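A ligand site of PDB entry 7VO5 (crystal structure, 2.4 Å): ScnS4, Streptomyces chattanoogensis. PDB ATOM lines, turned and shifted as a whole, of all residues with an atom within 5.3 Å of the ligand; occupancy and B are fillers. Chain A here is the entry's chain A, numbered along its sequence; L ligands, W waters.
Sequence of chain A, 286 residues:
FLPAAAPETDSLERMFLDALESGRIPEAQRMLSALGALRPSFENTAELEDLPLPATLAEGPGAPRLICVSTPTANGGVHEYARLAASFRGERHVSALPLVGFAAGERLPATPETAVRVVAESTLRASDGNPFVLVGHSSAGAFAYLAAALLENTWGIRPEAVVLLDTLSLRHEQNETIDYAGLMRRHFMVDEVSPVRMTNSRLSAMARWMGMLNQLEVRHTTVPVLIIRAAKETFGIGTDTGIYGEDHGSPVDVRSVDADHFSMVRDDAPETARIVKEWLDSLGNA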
ATOM      1  N   GLN A  29       9.165  -8.925  -4.257  1.00  0.00           N
ATOM      2  CA  GLN A  29       8.234  -9.791  -3.526  1.00  0.00           C
ATOM      3  C   GLN A  29       8.673 -11.217  -3.443  1.00  0.00           C
ATOM      4  O   GLN A  29       8.583 -11.853  -2.357  1.00  0.00           O
ATOM      5  CB  GLN A  29       6.821  -9.712  -4.136  1.00  0.00           C
ATOM      6  CG  GLN A  29       6.024  -8.528  -3.583  1.00  0.00           C
ATOM      7  CD  GLN A  29       4.569  -8.421  -4.076  1.00  0.00           C
ATOM      8  OE1 GLN A  29       3.691  -7.945  -3.345  1.00  0.00           O
ATOM      9  NE2 GLN A  29       4.341  -8.806  -5.326  1.00  0.00           N
ATOM     10  N   ARG A  30       9.121 -11.724  -4.571  1.00  0.00           N
ATOM     11  CA  ARG A  30       9.605 -13.086  -4.621  1.00  0.00           C
ATOM     12  C   ARG A  30      10.851 -13.267  -3.722  1.00  0.00           C
ATOM     13  O   ARG A  30      10.965 -14.255  -2.995  1.00  0.00           O
ATOM     14  CB  ARG A  30       9.904 -13.465  -6.050  1.00  0.00           C
ATOM     15  CG  ARG A  30       9.890 -14.960  -6.309  1.00  0.00           C
ATOM     16  CD  ARG A  30      10.038 -15.287  -7.794  1.00  0.00           C
ATOM     17  NE  ARG A  30       9.231 -14.394  -8.693  1.00  0.00           N
ATOM     18  CZ  ARG A  30       9.696 -13.384  -9.450  1.00  0.00           C
ATOM     19  NH1 ARG A  30      11.004 -13.038  -9.468  1.00  0.00           N
ATOM     20  NH2 ARG A  30       8.858 -12.680 -10.194  1.00  0.00           N
ATOM     21  N   LEU A  32      11.499 -11.595  -0.996  1.00  0.00           N
ATOM     22  CA  LEU A  32      10.939 -11.544   0.362  1.00  0.00           C
ATOM     23  C   LEU A  32      10.319 -12.858   0.769  1.00  0.00           C
ATOM     24  O   LEU A  32      10.526 -13.353   1.849  1.00  0.00           O
ATOM     25  CB  LEU A  32       9.882 -10.445   0.406  1.00  0.00           C
ATOM     26  CG  LEU A  32      10.069  -9.118   1.126  1.00  0.00           C
ATOM     27  CD1 LEU A  32      11.511  -8.717   1.287  1.00  0.00           C
ATOM     28  CD2 LEU A  32       9.227  -8.068   0.411  1.00  0.00           C
ATOM     29  N   SER A  33       9.591 -13.439  -0.170  1.00  0.00           N
ATOM     30  CA  SER A  33       8.918 -14.688   0.087  1.00  0.00           C
ATOM     31  C   SER A  33       9.902 -15.847   0.317  1.00  0.00           C
ATOM     32  O   SER A  33       9.816 -16.629   1.258  1.00  0.00           O
ATOM     33  CB  SER A  33       8.061 -14.976  -1.131  1.00  0.00           C
ATOM     34  OG  SER A  33       7.488 -16.231  -0.953  1.00  0.00           O
ATOM     35  N   THR A  71       1.880  -2.369  12.191  1.00  0.00           N
ATOM     36  CA  THR A  71       1.685  -2.837  10.844  1.00  0.00           C
ATOM     37  C   THR A  71       2.753  -3.844  10.546  1.00  0.00           C
ATOM     38  O   THR A  71       3.874  -3.698  10.984  1.00  0.00           O
ATOM     39  CB  THR A  71       1.736  -1.650   9.865  1.00  0.00           C
ATOM     40  OG1 THR A  71       0.736  -0.700  10.257  1.00  0.00           O
ATOM     41  CG2 THR A  71       1.468  -2.046   8.449  1.00  0.00           C
ATOM     42  N   THR A  73       4.867  -4.293   8.464  1.00  0.00           N
ATOM     43  CA  THR A  73       5.846  -3.771   7.558  1.00  0.00           C
ATOM     44  C   THR A  73       7.226  -3.881   8.145  1.00  0.00           C
ATOM     45  O   THR A  73       7.385  -3.853   9.333  1.00  0.00           O
ATOM     46  CB  THR A  73       5.539  -2.293   7.279  1.00  0.00           C
ATOM     47  OG1 THR A  73       5.064  -1.661   8.462  1.00  0.00           O
ATOM     48  CG2 THR A  73       4.512  -2.169   6.188  1.00  0.00           C
ATOM     49  N   SER A 138      -3.931   0.352   8.446  1.00  0.00           N
ATOM     50  CA  SER A 138      -3.853  -0.482   7.242  1.00  0.00           C
ATOM     51  C   SER A 138      -4.121  -1.906   7.614  1.00  0.00           C
ATOM     52  O   SER A 138      -5.104  -2.155   8.263  1.00  0.00           O
ATOM     53  CB  SER A 138      -2.536  -0.264   6.443  1.00  0.00           C
ATOM     54  OG  SER A 138      -2.633  -0.778   5.102  1.00  0.00           O
ATOM     55  N   SER A 139      -3.225  -2.821   7.299  1.00  0.00           N
ATOM     56  CA  SER A 139      -3.444  -4.214   7.512  1.00  0.00           C
ATOM     57  C   SER A 139      -3.337  -4.601   8.969  1.00  0.00           C
ATOM     58  O   SER A 139      -3.789  -5.693   9.384  1.00  0.00           O
ATOM     59  CB  SER A 139      -2.445  -4.991   6.678  1.00  0.00           C
ATOM     60  OG  SER A 139      -1.103  -4.697   7.066  1.00  0.00           O
ATOM     61  N   HIS A 172      -6.692  -9.113   2.059  1.00  0.00           N
ATOM     62  CA  HIS A 172      -5.819  -8.416   1.131  1.00  0.00           C
ATOM     63  C   HIS A 172      -5.513  -9.258  -0.050  1.00  0.00           C
ATOM     64  O   HIS A 172      -4.378  -9.380  -0.478  1.00  0.00           O
ATOM     65  CB  HIS A 172      -4.592  -7.835   1.826  1.00  0.00           C
ATOM     66  CG  HIS A 172      -4.896  -6.815   2.873  1.00  0.00           C
ATOM     67  ND1 HIS A 172      -5.309  -7.155   4.143  1.00  0.00           N
ATOM     68  CD2 HIS A 172      -4.834  -5.466   2.842  1.00  0.00           C
ATOM     69  CE1 HIS A 172      -5.498  -6.055   4.840  1.00  0.00           C
ATOM     70  NE2 HIS A 172      -5.221  -5.018   4.087  1.00  0.00           N
ATOM     71  N   GLN A 174      -4.982 -10.436  -3.616  1.00  0.00           N
ATOM     72  CA  GLN A 174      -4.438  -9.730  -4.744  1.00  0.00           C
ATOM     73  C   GLN A 174      -5.381  -9.951  -5.867  1.00  0.00           C
ATOM     74  O   GLN A 174      -5.359 -10.995  -6.489  1.00  0.00           O
ATOM     75  CB  GLN A 174      -3.037 -10.241  -5.037  1.00  0.00           C
ATOM     76  CG  GLN A 174      -2.183 -10.400  -3.789  1.00  0.00           C
ATOM     77  CD  GLN A 174      -1.624  -9.073  -3.300  1.00  0.00           C
ATOM     78  OE1 GLN A 174      -2.065  -8.542  -2.283  1.00  0.00           O
ATOM     79  NE2 GLN A 174      -0.655  -8.546  -4.018  1.00  0.00           N
ATOM     80  N   TYR A 180      -2.153  -2.900  -4.876  1.00  0.00           N
ATOM     81  CA  TYR A 180      -1.349  -3.318  -3.708  1.00  0.00           C
ATOM     82  C   TYR A 180       0.145  -3.019  -3.961  1.00  0.00           C
ATOM     83  O   TYR A 180       0.831  -2.436  -3.112  1.00  0.00           O
ATOM     84  CB  TYR A 180      -1.609  -4.805  -3.359  1.00  0.00           C
ATOM     85  CG  TYR A 180      -2.942  -5.039  -2.645  1.00  0.00           C
ATOM     86  CD1 TYR A 180      -3.178  -4.517  -1.400  1.00  0.00           C
ATOM     87  CD2 TYR A 180      -3.943  -5.803  -3.220  1.00  0.00           C
ATOM     88  CE1 TYR A 180      -4.385  -4.703  -0.740  1.00  0.00           C
ATOM     89  CE2 TYR A 180      -5.151  -6.034  -2.572  1.00  0.00           C
ATOM     90  CZ  TYR A 180      -5.392  -5.472  -1.322  1.00  0.00           C
ATOM     91  OH  TYR A 180      -6.613  -5.628  -0.656  1.00  0.00           O
ATOM     92  N   LEU A 183       0.794   0.679  -3.561  1.00  0.00           N
ATOM     93  CA  LEU A 183       0.725   1.007  -2.157  1.00  0.00           C
ATOM     94  C   LEU A 183       2.063   0.604  -1.398  1.00  0.00           C
ATOM     95  O   LEU A 183       2.495   1.297  -0.498  1.00  0.00           O
ATOM     96  CB  LEU A 183      -0.497   0.316  -1.557  1.00  0.00           C
ATOM     97  CG  LEU A 183      -1.014   0.865  -0.230  1.00  0.00           C
ATOM     98  CD1 LEU A 183      -1.606   2.264  -0.382  1.00  0.00           C
ATOM     99  CD2 LEU A 183      -2.024  -0.117   0.315  1.00  0.00           C
ATOM    100  N   MET A 184       2.673  -0.499  -1.795  1.00  0.00           N
ATOM    101  CA  MET A 184       3.914  -0.959  -1.219  1.00  0.00           C
ATOM    102  C   MET A 184       5.034   0.034  -1.588  1.00  0.00           C
ATOM    103  O   MET A 184       5.826   0.443  -0.718  1.00  0.00           O
ATOM    104  CB  MET A 184       4.227  -2.362  -1.740  1.00  0.00           C
ATOM    105  CG  MET A 184       5.534  -3.046  -1.261  1.00  0.00           C
ATOM    106  SD  MET A 184       5.746  -4.551  -2.256  1.00  0.00           S
ATOM    107  CE  MET A 184       6.928  -5.425  -1.240  1.00  0.00           C
ATOM    108  N   HIS A 187       4.499   3.263   0.415  1.00  0.00           N
ATOM    109  CA  HIS A 187       4.840   3.139   1.827  1.00  0.00           C
ATOM    110  C   HIS A 187       6.348   3.306   2.069  1.00  0.00           C
ATOM    111  O   HIS A 187       6.761   4.053   2.942  1.00  0.00           O
ATOM    112  CB  HIS A 187       4.400   1.771   2.378  1.00  0.00           C
ATOM    113  CG  HIS A 187       4.857   1.541   3.792  1.00  0.00           C
ATOM    114  ND1 HIS A 187       4.229   2.113   4.865  1.00  0.00           N
ATOM    115  CD2 HIS A 187       5.938   0.887   4.279  1.00  0.00           C
ATOM    116  CE1 HIS A 187       4.889   1.806   5.973  1.00  0.00           C
ATOM    117  NE2 HIS A 187       5.926   1.058   5.639  1.00  0.00           N
ATOM    118  N   PHE A 188       7.123   2.568   1.264  1.00  0.00           N
ATOM    119  CA  PHE A 188       8.572   2.507   1.408  1.00  0.00           C
ATOM    120  C   PHE A 188       9.289   3.688   0.748  1.00  0.00           C
ATOM    121  O   PHE A 188      10.428   3.929   1.057  1.00  0.00           O
ATOM    122  CB  PHE A 188       9.111   1.157   0.879  1.00  0.00           C
ATOM    123  CG  PHE A 188       8.769   0.009   1.773  1.00  0.00           C
ATOM    124  CD1 PHE A 188       9.288  -0.067   3.013  1.00  0.00           C
ATOM    125  CD2 PHE A 188       7.884  -0.970   1.376  1.00  0.00           C
ATOM    126  CE1 PHE A 188       8.945  -1.067   3.869  1.00  0.00           C
ATOM    127  CE2 PHE A 188       7.527  -1.969   2.229  1.00  0.00           C
ATOM    128  CZ  PHE A 188       8.080  -2.025   3.483  1.00  0.00           C
ATOM    129  N   MET A 206       8.073  -9.324   7.626  1.00  0.00           N
ATOM    130  CA  MET A 206       7.133  -8.759   6.723  1.00  0.00           C
ATOM    131  C   MET A 206       6.623  -9.782   5.714  1.00  0.00           C
ATOM    132  O   MET A 206       5.409  -9.965   5.550  1.00  0.00           O
ATOM    133  CB  MET A 206       7.686  -7.554   5.994  1.00  0.00           C
ATOM    134  CG  MET A 206       6.820  -7.182   4.796  1.00  0.00           C
ATOM    135  SD  MET A 206       7.073  -5.494   4.383  1.00  0.00           S
ATOM    136  CE  MET A 206       8.703  -5.660   3.686  1.00  0.00           C
ATOM    137  N   ALA A 207       7.473 -10.483   5.002  1.00  0.00           N
ATOM    138  CA  ALA A 207       6.956 -11.423   4.047  1.00  0.00           C
ATOM    139  C   ALA A 207       6.018 -12.453   4.641  1.00  0.00           C
ATOM    140  O   ALA A 207       4.977 -12.708   4.112  1.00  0.00           O
ATOM    141  CB  ALA A 207       8.077 -12.083   3.372  1.00  0.00           C
ATOM    142  N   MET A 210       2.766 -10.647   5.905  1.00  0.00           N
ATOM    143  CA  MET A 210       1.929 -10.225   4.784  1.00  0.00           C
ATOM    144  C   MET A 210       1.385 -11.433   4.065  1.00  0.00           C
ATOM    145  O   MET A 210       0.282 -11.390   3.549  1.00  0.00           O
ATOM    146  CB  MET A 210       2.649  -9.341   3.790  1.00  0.00           C
ATOM    147  CG  MET A 210       3.034  -7.981   4.279  1.00  0.00           C
ATOM    148  SD  MET A 210       1.637  -6.994   4.897  1.00  0.00           S
ATOM    149  CE  MET A 210       2.392  -5.387   5.117  1.00  0.00           C
ATOM    150  N   GLY A 211       2.170 -12.502   3.975  1.00  0.00           N
ATOM    151  CA  GLY A 211       1.775 -13.694   3.223  1.00  0.00           C
ATOM    152  C   GLY A 211       0.602 -14.386   3.890  1.00  0.00           C
ATOM    153  O   GLY A 211      -0.207 -14.997   3.206  1.00  0.00           O
ATOM    154  N   LEU A 213      -1.919 -12.828   5.493  1.00  0.00           N
ATOM    155  CA  LEU A 213      -3.189 -12.137   5.218  1.00  0.00           C
ATOM    156  C   LEU A 213      -4.146 -12.975   4.329  1.00  0.00           C
ATOM    157  O   LEU A 213      -5.308 -13.200   4.677  1.00  0.00           O
ATOM    158  CB  LEU A 213      -2.973 -10.741   4.607  1.00  0.00           C
ATOM    159  CG  LEU A 213      -2.240  -9.698   5.488  1.00  0.00           C
ATOM    160  CD1 LEU A 213      -2.099  -8.380   4.804  1.00  0.00           C
ATOM    161  CD2 LEU A 213      -2.937  -9.455   6.775  1.00  0.00           C
ATOM    162  N   ASN A 214      -3.669 -13.494   3.200  1.00  0.00           N
ATOM    163  CA  ASN A 214      -4.529 -14.218   2.249  1.00  0.00           C
ATOM    164  C   ASN A 214      -5.199 -15.461   2.765  1.00  0.00           C
ATOM    165  O   ASN A 214      -6.155 -15.920   2.187  1.00  0.00           O
ATOM    166  CB  ASN A 214      -3.726 -14.538   0.984  1.00  0.00           C
ATOM    167  CG  ASN A 214      -3.364 -13.305   0.179  1.00  0.00           C
ATOM    168  OD1 ASN A 214      -3.260 -12.209   0.697  1.00  0.00           O
ATOM    169  ND2 ASN A 214      -3.152 -13.503  -1.114  1.00  0.00           N
ATOM    170  N   GLN A 215      -4.722 -16.006   3.860  1.00  0.00           N
ATOM    171  CA  GLN A 215      -5.243 -17.236   4.394  1.00  0.00           C
ATOM    172  C   GLN A 215      -5.814 -17.100   5.791  1.00  0.00           C
ATOM    173  O   GLN A 215      -5.951 -18.089   6.493  1.00  0.00           O
ATOM    174  CB  GLN A 215      -4.142 -18.268   4.365  1.00  0.00           C
ATOM    175  CG  GLN A 215      -2.754 -17.690   4.534  1.00  0.00           C
ATOM    176  CD  GLN A 215      -1.786 -18.101   3.459  1.00  0.00           C
ATOM    177  OE1 GLN A 215      -2.075 -17.995   2.274  1.00  0.00           O
ATOM    178  NE2 GLN A 215      -0.609 -18.571   3.875  1.00  0.00           N
ATOM    179  N   HIS A 261      -3.722   7.752   3.052  1.00  0.00           N
ATOM    180  CA  HIS A 261      -3.428   6.532   3.805  1.00  0.00           C
ATOM    181  C   HIS A 261      -2.245   6.664   4.755  1.00  0.00           C
ATOM    182  O   HIS A 261      -2.266   6.168   5.871  1.00  0.00           O
ATOM    183  CB  HIS A 261      -3.154   5.421   2.766  1.00  0.00           C
ATOM    184  CG  HIS A 261      -2.986   4.045   3.364  1.00  0.00           C
ATOM    185  ND1 HIS A 261      -4.043   3.197   3.580  1.00  0.00           N
ATOM    186  CD2 HIS A 261      -1.874   3.357   3.714  1.00  0.00           C
ATOM    187  CE1 HIS A 261      -3.600   2.051   4.053  1.00  0.00           C
ATOM    188  NE2 HIS A 261      -2.287   2.112   4.135  1.00  0.00           N
ATOM    189  N   PHE A 262      -1.243   7.391   4.317  1.00  0.00           N
ATOM    190  CA  PHE A 262      -0.016   7.650   5.066  1.00  0.00           C
ATOM    191  C   PHE A 262      -0.164   8.893   5.933  1.00  0.00           C
ATOM    192  O   PHE A 262       0.053   8.857   7.166  1.00  0.00           O
ATOM    193  CB  PHE A 262       1.157   7.709   4.067  1.00  0.00           C
ATOM    194  CG  PHE A 262       1.211   6.507   3.179  1.00  0.00           C
ATOM    195  CD1 PHE A 262       1.588   5.282   3.686  1.00  0.00           C
ATOM    196  CD2 PHE A 262       0.825   6.564   1.870  1.00  0.00           C
ATOM    197  CE1 PHE A 262       1.636   4.144   2.900  1.00  0.00           C
ATOM    198  CE2 PHE A 262       0.854   5.438   1.076  1.00  0.00           C
ATOM    199  CZ  PHE A 262       1.238   4.211   1.610  1.00  0.00           C
HETATM  200  O1  LIG L   1      -0.342  -3.065   4.890  1.00  0.00           O
HETATM  201  C1  LIG L   1      -0.377  -3.327   3.721  1.00  0.00           C
HETATM  202  C2  LIG L   1      -1.060  -4.585   3.250  1.00  0.00           C
HETATM  203  C3  LIG L   1      -0.443  -5.030   1.933  1.00  0.00           C
HETATM  204  O2  LIG L   1      -0.930  -4.132   0.950  1.00  0.00           O
HETATM  205  C4  LIG L   1      -0.890  -6.410   1.541  1.00  0.00           C
HETATM  206  C5  LIG L   1      -0.020  -7.400   1.396  1.00  0.00           C
HETATM  207  C6  LIG L   1      -0.516  -8.771   0.997  1.00  0.00           C
HETATM  208  C7  LIG L   1       0.574  -9.531   0.271  1.00  0.00           C
HETATM  209  O3  LIG L   1       0.867  -8.880  -0.953  1.00  0.00           O
HETATM  210  C8  LIG L   1       0.059 -10.923  -0.059  1.00  0.00           C
HETATM  211  C9  LIG L   1       1.122 -11.835  -0.664  1.00  0.00           C
HETATM  212  O4  LIG L   1       1.467 -11.395  -1.979  1.00  0.00           O
HETATM  213  O5  LIG L   1       2.274 -11.838   0.166  1.00  0.00           O
HETATM  214  C10 LIG L   1       3.330 -12.650  -0.348  1.00  0.00           C
HETATM  215  C11 LIG L   1       2.886 -14.101  -0.304  1.00  0.00           C
HETATM  216  C12 LIG L   1       3.935 -15.049  -0.865  1.00  0.00           C
HETATM  217  C13 LIG L   1       1.571 -14.309  -1.039  1.00  0.00           C
HETATM  218  O6  LIG L   1       1.016 -15.557  -0.638  1.00  0.00           O
HETATM  219  C14 LIG L   1       0.544 -13.231  -0.711  1.00  0.00           C
HETATM  220  C15 LIG L   1       4.566 -12.435   0.528  1.00  0.00           C
HETATM  221  C16 LIG L   1       5.566 -11.493  -0.106  1.00  0.00           C
HETATM  222  O7  LIG L   1       5.873 -12.003  -1.400  1.00  0.00           O
HETATM  223  C17 LIG L   1       4.896 -10.155  -0.226  1.00  0.00           C
HETATM  224  C18 LIG L   1       5.223  -9.141   0.546  1.00  0.00           C
HETATM  225  C19 LIG L   1       4.486  -7.912   0.370  1.00  0.00           C
HETATM  226  C20 LIG L   1       4.652  -6.917   1.223  1.00  0.00           C
HETATM  227  C21 LIG L   1       3.883  -5.716   1.053  1.00  0.00           C
HETATM  228  C22 LIG L   1       4.110  -4.686   1.848  1.00  0.00           C
HETATM  229  C23 LIG L   1       3.314  -3.494   1.663  1.00  0.00           C
HETATM  230  C24 LIG L   1       3.250  -2.586   2.626  1.00  0.00           C
HETATM  231  C25 LIG L   1       2.400  -1.373   2.429  1.00  0.00           C
HETATM  232  C26 LIG L   1       1.166  -1.473   3.309  1.00  0.00           C
HETATM  233  O8  LIG L   1       0.268  -2.436   2.762  1.00  0.00           O
HETATM  234  C27 LIG L   1       0.483  -0.119   3.305  1.00  0.00           C
HETATM  235  O   HOH W   1       1.118   1.702   5.804  1.00  0.00           O
HETATM  236  O   HOH W   2       1.432  -6.550  -2.139  1.00  0.00           O
HETATM  237  O   HOH W   3       5.727 -14.877   2.379  1.00  0.00           O
HETATM  238  O   HOH W   4       0.958  -4.242  -0.885  1.00  0.00           O
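OG of Ser 139 is in hydrogen-bond range of O1 of the ligand (2.8 Å).
O of Gln 29 sits at hydrogen-bond distance from O7 of the ligand, at 2.9 Å.
O3 of the ligand lies within hydrogen-bond range of OE1 of Gln 174.
An oxygen (O1) of the ligand lies within hydrogen-bond range of the side-chain hydroxyl (OG) of Ser 138, at 3.2 Å.
The backbone carbonyl oxygen of His 172 lies close to the side-chain amide oxygen of Gln 174.
OG of Ser 138 lies within hydrogen-bond range of NE2 of His 261, at 3.1 Å.
The side-chain amide oxygen (OD1) of Asn 214 sits close to the backbone carbonyl oxygen (O) of His 172.
The side-chain hydroxyl (OG1) of Thr 73 lies within hydrogen-bond range of the backbone carbonyl oxygen (O) of Thr 71, 3.5 Å away.
Merely in contact with the ligand: Ser 33 (3.7 Å), Thr 73 (3.8 Å), His 172 (3.9 Å), Tyr 180 (3.3 Å), Leu 183 (3.9 Å), Met 184 (3.7 Å), His 187 (3.7 Å), Met 206 (3.98 Å), Ala 207 (3.6 Å), Met 210 (3.6 Å), Gly 211 (3.6 Å), Leu 213 (3.999 Å), Asn 214 (3.6 Å) and His 261 (3.7 Å).
Of the 24 residues printed, 18 come within 4 Å of the ligand.
Along chain A the residues within 4 Å of the ligand span positions 29 to 261.
The nearest printed residue that does not touch the ligand is Thr 71 (4.1 Å).
Water W4 bridges an oxygen (O2) of the ligand (2.6 Å) and the backbone carbonyl oxygen (O) of Tyr 180 (2.9 Å).
Water W2 lies within hydrogen-bond range of an oxygen (O3) of the ligand (2.7 Å), the side-chain amide oxygen (OE1) of Gln 29 (2.9 Å) and the side-chain amide nitrogen (NE2) of Gln 174 (3.4 Å).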
